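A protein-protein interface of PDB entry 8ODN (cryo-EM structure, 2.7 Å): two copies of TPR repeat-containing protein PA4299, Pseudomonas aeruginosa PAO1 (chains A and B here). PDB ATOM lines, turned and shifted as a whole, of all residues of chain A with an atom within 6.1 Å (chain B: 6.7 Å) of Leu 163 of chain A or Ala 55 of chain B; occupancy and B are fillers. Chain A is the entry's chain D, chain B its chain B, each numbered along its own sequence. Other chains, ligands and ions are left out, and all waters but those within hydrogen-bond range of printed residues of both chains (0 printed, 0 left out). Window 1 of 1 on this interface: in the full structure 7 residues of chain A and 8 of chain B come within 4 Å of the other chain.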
ATOM      1  N   PRO A 131       4.142  -0.614  -8.027  1.00  0.00           N
ATOM      2  CA  PRO A 131       4.197  -1.418  -6.795  1.00  0.00           C
ATOM      3  C   PRO A 131       5.091  -0.853  -5.707  1.00  0.00           C
ATOM      4  O   PRO A 131       4.740  -0.945  -4.525  1.00  0.00           O
ATOM      5  CB  PRO A 131       4.720  -2.773  -7.295  1.00  0.00           C
ATOM      6  CG  PRO A 131       4.482  -2.774  -8.762  1.00  0.00           C
ATOM      7  CD  PRO A 131       4.637  -1.363  -9.192  1.00  0.00           C
ATOM      8  N   THR A 132       6.242  -0.279  -6.059  1.00  0.00           N
ATOM      9  CA  THR A 132       7.228   0.072  -5.043  1.00  0.00           C
ATOM     10  C   THR A 132       6.751   1.172  -4.105  1.00  0.00           C
ATOM     11  O   THR A 132       7.414   1.425  -3.095  1.00  0.00           O
ATOM     12  CB  THR A 132       8.540   0.506  -5.703  1.00  0.00           C
ATOM     13  OG1 THR A 132       9.530   0.734  -4.692  1.00  0.00           O
ATOM     14  CG2 THR A 132       8.344   1.784  -6.514  1.00  0.00           C
ATOM     15  N   GLU A 133       5.631   1.826  -4.408  1.00  0.00           N
ATOM     16  CA  GLU A 133       5.142   2.915  -3.573  1.00  0.00           C
ATOM     17  C   GLU A 133       4.698   2.389  -2.214  1.00  0.00           C
ATOM     18  O   GLU A 133       3.649   1.748  -2.097  1.00  0.00           O
ATOM     19  CB  GLU A 133       3.985   3.648  -4.256  1.00  0.00           C
ATOM     20  CG  GLU A 133       3.629   4.959  -3.574  1.00  0.00           C
ATOM     21  CD  GLU A 133       4.772   5.956  -3.622  1.00  0.00           C
ATOM     22  OE1 GLU A 133       5.637   5.821  -4.512  1.00  0.00           O
ATOM     23  OE2 GLU A 133       4.812   6.864  -2.765  1.00  0.00           O
ATOM     24  N   SER A 134       5.499   2.661  -1.179  1.00  0.00           N
ATOM     25  CA  SER A 134       5.172   2.210   0.172  1.00  0.00           C
ATOM     26  C   SER A 134       3.822   2.758   0.619  1.00  0.00           C
ATOM     27  O   SER A 134       3.038   2.061   1.271  1.00  0.00           O
ATOM     28  CB  SER A 134       6.273   2.638   1.145  1.00  0.00           C
ATOM     29  OG  SER A 134       5.964   2.258   2.475  1.00  0.00           O
ATOM     30  N   ARG A 137       1.014   0.682  -0.817  1.00  0.00           N
ATOM     31  CA  ARG A 137       0.921  -0.627  -0.180  1.00  0.00           C
ATOM     32  C   ARG A 137       0.315  -0.523   1.214  1.00  0.00           C
ATOM     33  O   ARG A 137      -0.539  -1.336   1.592  1.00  0.00           O
ATOM     34  CB  ARG A 137       2.307  -1.270  -0.124  1.00  0.00           C
ATOM     35  CG  ARG A 137       2.870  -1.637  -1.489  1.00  0.00           C
ATOM     36  CD  ARG A 137       2.210  -2.885  -2.044  1.00  0.00           C
ATOM     37  NE  ARG A 137       2.284  -2.950  -3.498  1.00  0.00           N
ATOM     38  CZ  ARG A 137       1.888  -3.987  -4.225  1.00  0.00           C
ATOM     39  NH1 ARG A 137       1.403  -5.081  -3.662  1.00  0.00           N
ATOM     40  NH2 ARG A 137       1.980  -3.924  -5.549  1.00  0.00           N
ATOM     41  N   ILE A 158       2.948  -6.266   4.980  1.00  0.00           N
ATOM     42  CA  ILE A 158       4.337  -6.706   4.969  1.00  0.00           C
ATOM     43  C   ILE A 158       5.085  -6.062   3.811  1.00  0.00           C
ATOM     44  O   ILE A 158       6.240  -5.650   3.957  1.00  0.00           O
ATOM     45  CB  ILE A 158       4.415  -8.242   4.918  1.00  0.00           C
ATOM     46  CG1 ILE A 158       3.855  -8.838   6.212  1.00  0.00           C
ATOM     47  CG2 ILE A 158       5.857  -8.684   4.706  1.00  0.00           C
ATOM     48  CD1 ILE A 158       3.549 -10.322   6.128  1.00  0.00           C
ATOM     49  N   THR A 159       4.447  -5.965   2.643  1.00  0.00           N
ATOM     50  CA  THR A 159       5.094  -5.287   1.523  1.00  0.00           C
ATOM     51  C   THR A 159       5.443  -3.850   1.893  1.00  0.00           C
ATOM     52  O   THR A 159       6.568  -3.388   1.660  1.00  0.00           O
ATOM     53  CB  THR A 159       4.197  -5.312   0.282  1.00  0.00           C
ATOM     54  OG1 THR A 159       3.057  -4.470   0.496  1.00  0.00           O
ATOM     55  CG2 THR A 159       3.730  -6.728  -0.037  1.00  0.00           C
ATOM     56  N   ALA A 160       4.485  -3.124   2.474  1.00  0.00           N
ATOM     57  CA  ALA A 160       4.732  -1.735   2.854  1.00  0.00           C
ATOM     58  C   ALA A 160       5.833  -1.634   3.906  1.00  0.00           C
ATOM     59  O   ALA A 160       6.727  -0.786   3.808  1.00  0.00           O
ATOM     60  CB  ALA A 160       3.439  -1.095   3.361  1.00  0.00           C
ATOM     61  N   LEU A 161       5.779  -2.490   4.929  1.00  0.00           N
ATOM     62  CA  LEU A 161       6.764  -2.438   6.004  1.00  0.00           C
ATOM     63  C   LEU A 161       8.160  -2.782   5.502  1.00  0.00           C
ATOM     64  O   LEU A 161       9.152  -2.244   6.007  1.00  0.00           O
ATOM     65  CB  LEU A 161       6.344  -3.386   7.129  1.00  0.00           C
ATOM     66  CG  LEU A 161       7.231  -3.481   8.373  1.00  0.00           C
ATOM     67  CD1 LEU A 161       7.546  -2.108   8.946  1.00  0.00           C
ATOM     68  CD2 LEU A 161       6.553  -4.348   9.423  1.00  0.00           C
ATOM     69  N   GLU A 162       8.260  -3.676   4.518  1.00  0.00           N
ATOM     70  CA  GLU A 162       9.559  -4.009   3.946  1.00  0.00           C
ATOM     71  C   GLU A 162      10.073  -2.880   3.060  1.00  0.00           C
ATOM     72  O   GLU A 162      11.269  -2.568   3.073  1.00  0.00           O
ATOM     73  CB  GLU A 162       9.461  -5.312   3.155  1.00  0.00           C
ATOM     74  CG  GLU A 162       9.068  -6.533   3.984  1.00  0.00           C
ATOM     75  CD  GLU A 162      10.215  -7.101   4.796  1.00  0.00           C
ATOM     76  OE1 GLU A 162      11.056  -6.314   5.279  1.00  0.00           O
ATOM     77  OE2 GLU A 162      10.275  -8.338   4.951  1.00  0.00           O
ATOM     78  N   LEU A 163       9.186  -2.262   2.276  1.00  0.00           N
ATOM     79  CA  LEU A 163       9.600  -1.150   1.425  1.00  0.00           C
ATOM     80  C   LEU A 163      10.202  -0.022   2.253  1.00  0.00           C
ATOM     81  O   LEU A 163      11.308   0.452   1.970  1.00  0.00           O
ATOM     82  CB  LEU A 163       8.407  -0.644   0.613  1.00  0.00           C
ATOM     83  CG  LEU A 163       8.030  -1.466  -0.622  1.00  0.00           C
ATOM     84  CD1 LEU A 163       6.633  -1.105  -1.104  1.00  0.00           C
ATOM     85  CD2 LEU A 163       9.046  -1.257  -1.733  1.00  0.00           C
ATOM     86  N   GLN A 164       9.483   0.424   3.279  1.00  0.00           N
ATOM     87  CA  GLN A 164       9.976   1.488   4.140  1.00  0.00           C
ATOM     88  C   GLN A 164      11.118   0.979   5.016  1.00  0.00           C
ATOM     89  O   GLN A 164      11.145  -0.183   5.427  1.00  0.00           O
ATOM     90  CB  GLN A 164       8.838   2.034   5.003  1.00  0.00           C
ATOM     91  CG  GLN A 164       9.154   3.332   5.731  1.00  0.00           C
ATOM     92  CD  GLN A 164       7.912   3.989   6.306  1.00  0.00           C
ATOM     93  OE1 GLN A 164       6.809   3.820   5.786  1.00  0.00           O
ATOM     94  NE2 GLN A 164       8.083   4.731   7.395  1.00  0.00           N
ATOM     95  N   GLN A 165      12.068   1.871   5.302  1.00  0.00           N
ATOM     96  CA  GLN A 165      13.261   1.522   6.074  1.00  0.00           C
ATOM     97  C   GLN A 165      12.865   1.343   7.537  1.00  0.00           C
ATOM     98  O   GLN A 165      13.070   2.212   8.388  1.00  0.00           O
ATOM     99  CB  GLN A 165      14.335   2.594   5.914  1.00  0.00           C
ATOM    100  CG  GLN A 165      15.041   2.577   4.567  1.00  0.00           C
ATOM    101  CD  GLN A 165      16.281   1.702   4.563  1.00  0.00           C
ATOM    102  OE1 GLN A 165      17.406   2.202   4.558  1.00  0.00           O
ATOM    103  NE2 GLN A 165      16.080   0.390   4.563  1.00  0.00           N
ATOM    104  N   GLY A 166      12.284   0.179   7.828  1.00  0.00           N
ATOM    105  CA  GLY A 166      11.804  -0.142   9.150  1.00  0.00           C
ATOM    106  C   GLY A 166      10.353   0.212   9.395  1.00  0.00           C
ATOM    107  O   GLY A 166       9.696  -0.445  10.210  1.00  0.00           O
ATOM    108  N   VAL B  44      16.627  -5.494  -6.633  1.00  0.00           N
ATOM    109  CA  VAL B  44      15.726  -6.635  -6.483  1.00  0.00           C
ATOM    110  C   VAL B  44      16.408  -7.741  -5.690  1.00  0.00           C
ATOM    111  O   VAL B  44      15.843  -8.281  -4.735  1.00  0.00           O
ATOM    112  CB  VAL B  44      15.253  -7.134  -7.860  1.00  0.00           C
ATOM    113  CG1 VAL B  44      14.683  -8.536  -7.746  1.00  0.00           C
ATOM    114  CG2 VAL B  44      14.208  -6.187  -8.424  1.00  0.00           C
ATOM    115  N   MET B  47      16.651  -6.932  -2.070  1.00  0.00           N
ATOM    116  CA  MET B  47      15.382  -7.199  -1.400  1.00  0.00           C
ATOM    117  C   MET B  47      15.182  -8.692  -1.167  1.00  0.00           C
ATOM    118  O   MET B  47      14.717  -9.103  -0.097  1.00  0.00           O
ATOM    119  CB  MET B  47      14.228  -6.622  -2.221  1.00  0.00           C
ATOM    120  CG  MET B  47      14.027  -5.123  -2.036  1.00  0.00           C
ATOM    121  SD  MET B  47      12.718  -4.438  -3.074  1.00  0.00           S
ATOM    122  CE  MET B  47      13.511  -4.443  -4.679  1.00  0.00           C
ATOM    123  N   GLY B  51      14.963 -10.510   3.021  1.00  0.00           N
ATOM    124  CA  GLY B  51      13.687 -10.950   3.543  1.00  0.00           C
ATOM    125  C   GLY B  51      12.512 -10.153   3.031  1.00  0.00           C
ATOM    126  O   GLY B  51      11.381 -10.385   3.478  1.00  0.00           O
ATOM    127  N   ARG B  52      12.745  -9.222   2.104  1.00  0.00           N
ATOM    128  CA  ARG B  52      11.709  -8.387   1.515  1.00  0.00           C
ATOM    129  C   ARG B  52      11.207  -8.953   0.193  1.00  0.00           C
ATOM    130  O   ARG B  52      10.937  -8.195  -0.746  1.00  0.00           O
ATOM    131  CB  ARG B  52      12.241  -6.967   1.325  1.00  0.00           C
ATOM    132  CG  ARG B  52      12.908  -6.396   2.574  1.00  0.00           C
ATOM    133  CD  ARG B  52      13.495  -5.015   2.343  1.00  0.00           C
ATOM    134  NE  ARG B  52      14.558  -5.029   1.347  1.00  0.00           N
ATOM    135  CZ  ARG B  52      15.404  -4.028   1.145  1.00  0.00           C
ATOM    136  NH1 ARG B  52      15.337  -2.913   1.854  1.00  0.00           N
ATOM    137  NH2 ARG B  52      16.337  -4.146   0.205  1.00  0.00           N
ATOM    138  N   LEU B  53      11.095 -10.280   0.100  1.00  0.00           N
ATOM    139  CA  LEU B  53      10.617 -10.956  -1.103  1.00  0.00           C
ATOM    140  C   LEU B  53       9.443 -10.225  -1.739  1.00  0.00           C
ATOM    141  O   LEU B  53       9.382 -10.098  -2.963  1.00  0.00           O
ATOM    142  CB  LEU B  53      10.210 -12.398  -0.781  1.00  0.00           C
ATOM    143  CG  LEU B  53      11.338 -13.406  -0.546  1.00  0.00           C
ATOM    144  CD1 LEU B  53      10.779 -14.726  -0.055  1.00  0.00           C
ATOM    145  CD2 LEU B  53      12.147 -13.641  -1.810  1.00  0.00           C
ATOM    146  N   HIS B  54       8.493  -9.769  -0.923  1.00  0.00           N
ATOM    147  CA  HIS B  54       7.291  -9.142  -1.463  1.00  0.00           C
ATOM    148  C   HIS B  54       7.608  -7.780  -2.073  1.00  0.00           C
ATOM    149  O   HIS B  54       7.085  -7.426  -3.137  1.00  0.00           O
ATOM    150  CB  HIS B  54       6.228  -9.015  -0.368  1.00  0.00           C
ATOM    151  CG  HIS B  54       5.911 -10.302   0.338  1.00  0.00           C
ATOM    152  ND1 HIS B  54       4.664 -10.572   0.859  1.00  0.00           N
ATOM    153  CD2 HIS B  54       6.678 -11.382   0.628  1.00  0.00           C
ATOM    154  CE1 HIS B  54       4.672 -11.766   1.426  1.00  0.00           C
ATOM    155  NE2 HIS B  54       5.883 -12.278   1.300  1.00  0.00           N
ATOM    156  N   ALA B  55       8.466  -6.998  -1.412  1.00  0.00           N
ATOM    157  CA  ALA B  55       8.928  -5.746  -2.002  1.00  0.00           C
ATOM    158  C   ALA B  55       9.724  -6.003  -3.275  1.00  0.00           C
ATOM    159  O   ALA B  55       9.638  -5.235  -4.241  1.00  0.00           O
ATOM    160  CB  ALA B  55       9.768  -4.969  -0.989  1.00  0.00           C
ATOM    161  N   ALA B  56      10.526  -7.071  -3.285  1.00  0.00           N
ATOM    162  CA  ALA B  56      11.222  -7.452  -4.508  1.00  0.00           C
ATOM    163  C   ALA B  56      10.230  -7.773  -5.616  1.00  0.00           C
ATOM    164  O   ALA B  56      10.451  -7.421  -6.779  1.00  0.00           O
ATOM    165  CB  ALA B  56      12.133  -8.650  -4.241  1.00  0.00           C
ATOM    166  N   LEU B  57       9.134  -8.450  -5.273  1.00  0.00           N
ATOM    167  CA  LEU B  57       8.083  -8.719  -6.247  1.00  0.00           C
ATOM    168  C   LEU B  57       7.489  -7.423  -6.774  1.00  0.00           C
ATOM    169  O   LEU B  57       7.231  -7.289  -7.973  1.00  0.00           O
ATOM    170  CB  LEU B  57       6.993  -9.580  -5.608  1.00  0.00           C
ATOM    171  CG  LEU B  57       6.354 -10.646  -6.494  1.00  0.00           C
ATOM    172  CD1 LEU B  57       7.437 -11.551  -7.040  1.00  0.00           C
ATOM    173  CD2 LEU B  57       5.318 -11.434  -5.708  1.00  0.00           C
ATOM    174  N   ALA B  58       7.249  -6.465  -5.881  1.00  0.00           N
ATOM    175  CA  ALA B  58       6.747  -5.160  -6.303  1.00  0.00           C
ATOM    176  C   ALA B  58       7.691  -4.519  -7.316  1.00  0.00           C
ATOM    177  O   ALA B  58       7.274  -4.095  -8.403  1.00  0.00           O
ATOM    178  CB  ALA B  58       6.575  -4.259  -5.078  1.00  0.00           C
ATOM    179  N   ASN B  59       8.978  -4.457  -6.975  1.00  0.00           N
ATOM    180  CA  ASN B  59       9.947  -3.800  -7.847  1.00  0.00           C
ATOM    181  C   ASN B  59      10.090  -4.537  -9.175  1.00  0.00           C
ATOM    182  O   ASN B  59      10.278  -3.906 -10.222  1.00  0.00           O
ATOM    183  CB  ASN B  59      11.290  -3.690  -7.127  1.00  0.00           C
ATOM    184  CG  ASN B  59      11.360  -2.477  -6.214  1.00  0.00           C
ATOM    185  OD1 ASN B  59      12.318  -1.703  -6.264  1.00  0.00           O
ATOM    186  ND2 ASN B  59      10.337  -2.298  -5.386  1.00  0.00           N
ATOM    187  N   LEU B  60      10.022  -5.870  -9.153  1.00  0.00           N
ATOM    188  CA  LEU B  60      10.015  -6.638 -10.395  1.00  0.00           C
ATOM    189  C   LEU B  60       8.789  -6.304 -11.236  1.00  0.00           C
ATOM    190  O   LEU B  60       8.889  -6.106 -12.453  1.00  0.00           O
ATOM    191  CB  LEU B  60      10.056  -8.132 -10.076  1.00  0.00           C
ATOM    192  CG  LEU B  60      11.381  -8.652  -9.521  1.00  0.00           C
ATOM    193  CD1 LEU B  60      11.163  -9.850  -8.607  1.00  0.00           C
ATOM    194  CD2 LEU B  60      12.300  -9.020 -10.674  1.00  0.00           C
ATOM    195  N   ILE B  77      10.215 -15.736  -5.852  1.00  0.00           N
ATOM    196  CA  ILE B  77       9.445 -15.078  -4.798  1.00  0.00           C
ATOM    197  C   ILE B  77       8.097 -15.764  -4.617  1.00  0.00           C
ATOM    198  O   ILE B  77       7.670 -16.046  -3.493  1.00  0.00           O
ATOM    199  CB  ILE B  77       9.271 -13.584  -5.113  1.00  0.00           C
ATOM    200  CG1 ILE B  77      10.619 -12.865  -5.051  1.00  0.00           C
ATOM    201  CG2 ILE B  77       8.284 -12.949  -4.144  1.00  0.00           C
ATOM    202  CD1 ILE B  77      10.964 -12.105  -6.306  1.00  0.00           C
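CB of Pro 131 of chain A touches O of Ala 58 of chain B (3.1 Å). His 54 of chain B touches Thr 159 of chain A. Arg 52 of chain B touches Glu 162 of chain A (CG to OE1, 3.3 Å). Leu 163 of chain A touches Ala 55 of chain B (CD2 to CB, 3.9 Å).
Ala 55 of chain B touches just one residue of chain A: Leu 163 (3.9 Å). Of the printed residues of chain B, Thr 159 of chain A touches His 54. Of the printed residues of chain A, Gly 51 of chain B touches Glu 162 (2.8 Å). Printed residues of chain A within 4 Å of Arg 52 of chain B: Glu 162. Of the printed residues of chain A, Asn 59 of chain B touches Thr 132. Arg 137 of chain A touches none of the printed residues of chain B. The nearest printed residue of chain B that does not touch Leu 163 of chain A is Asn 59 of chain B (4.01 Å).
No position is printed for both chains.
The backbone carbonyl oxygen (O) of Pro 131 of chain A lies within hydrogen-bond range of the guanidinium group (NE) of Arg 137 of chain A, at 3.3 Å. O of Ala 55 of chain B lies within hydrogen-bond range of ND2 of Asn 59 of chain B, at 3.2 Å. The backbone carbonyl oxygen (O) of Met 47 of chain B lies within hydrogen-bond range of the backbone NH (N) of Arg 52 of chain B, at 3.0 Å.
Of the 14 printed residues of chain A, 5 touch a printed residue of chain B. Printed residues of chain A that touch a printed residue of chain B: Pro 131, Thr 132, Thr 159, Glu 162 and Leu 163. Along chain A the printed residues that touch a printed residue of chain B span positions 131 to 163. Hydrophobic or aromatic side chains of chain B that line the printed part of chain A: His 54, Ala 55 and Ala 58. Among the printed residues, 6 pairs touch across the chains.
The backbone carbonyl oxygen (O) of Gly 51 of chain B sits close to the side-chain carboxylate (OE2) of Glu 162 of chain A (2.8 Å). The side-chain hydroxyl of Thr 132 of chain A lies within hydrogen-bond range of the side-chain amide nitrogen of Asn 59 of chain B (3.2 Å).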
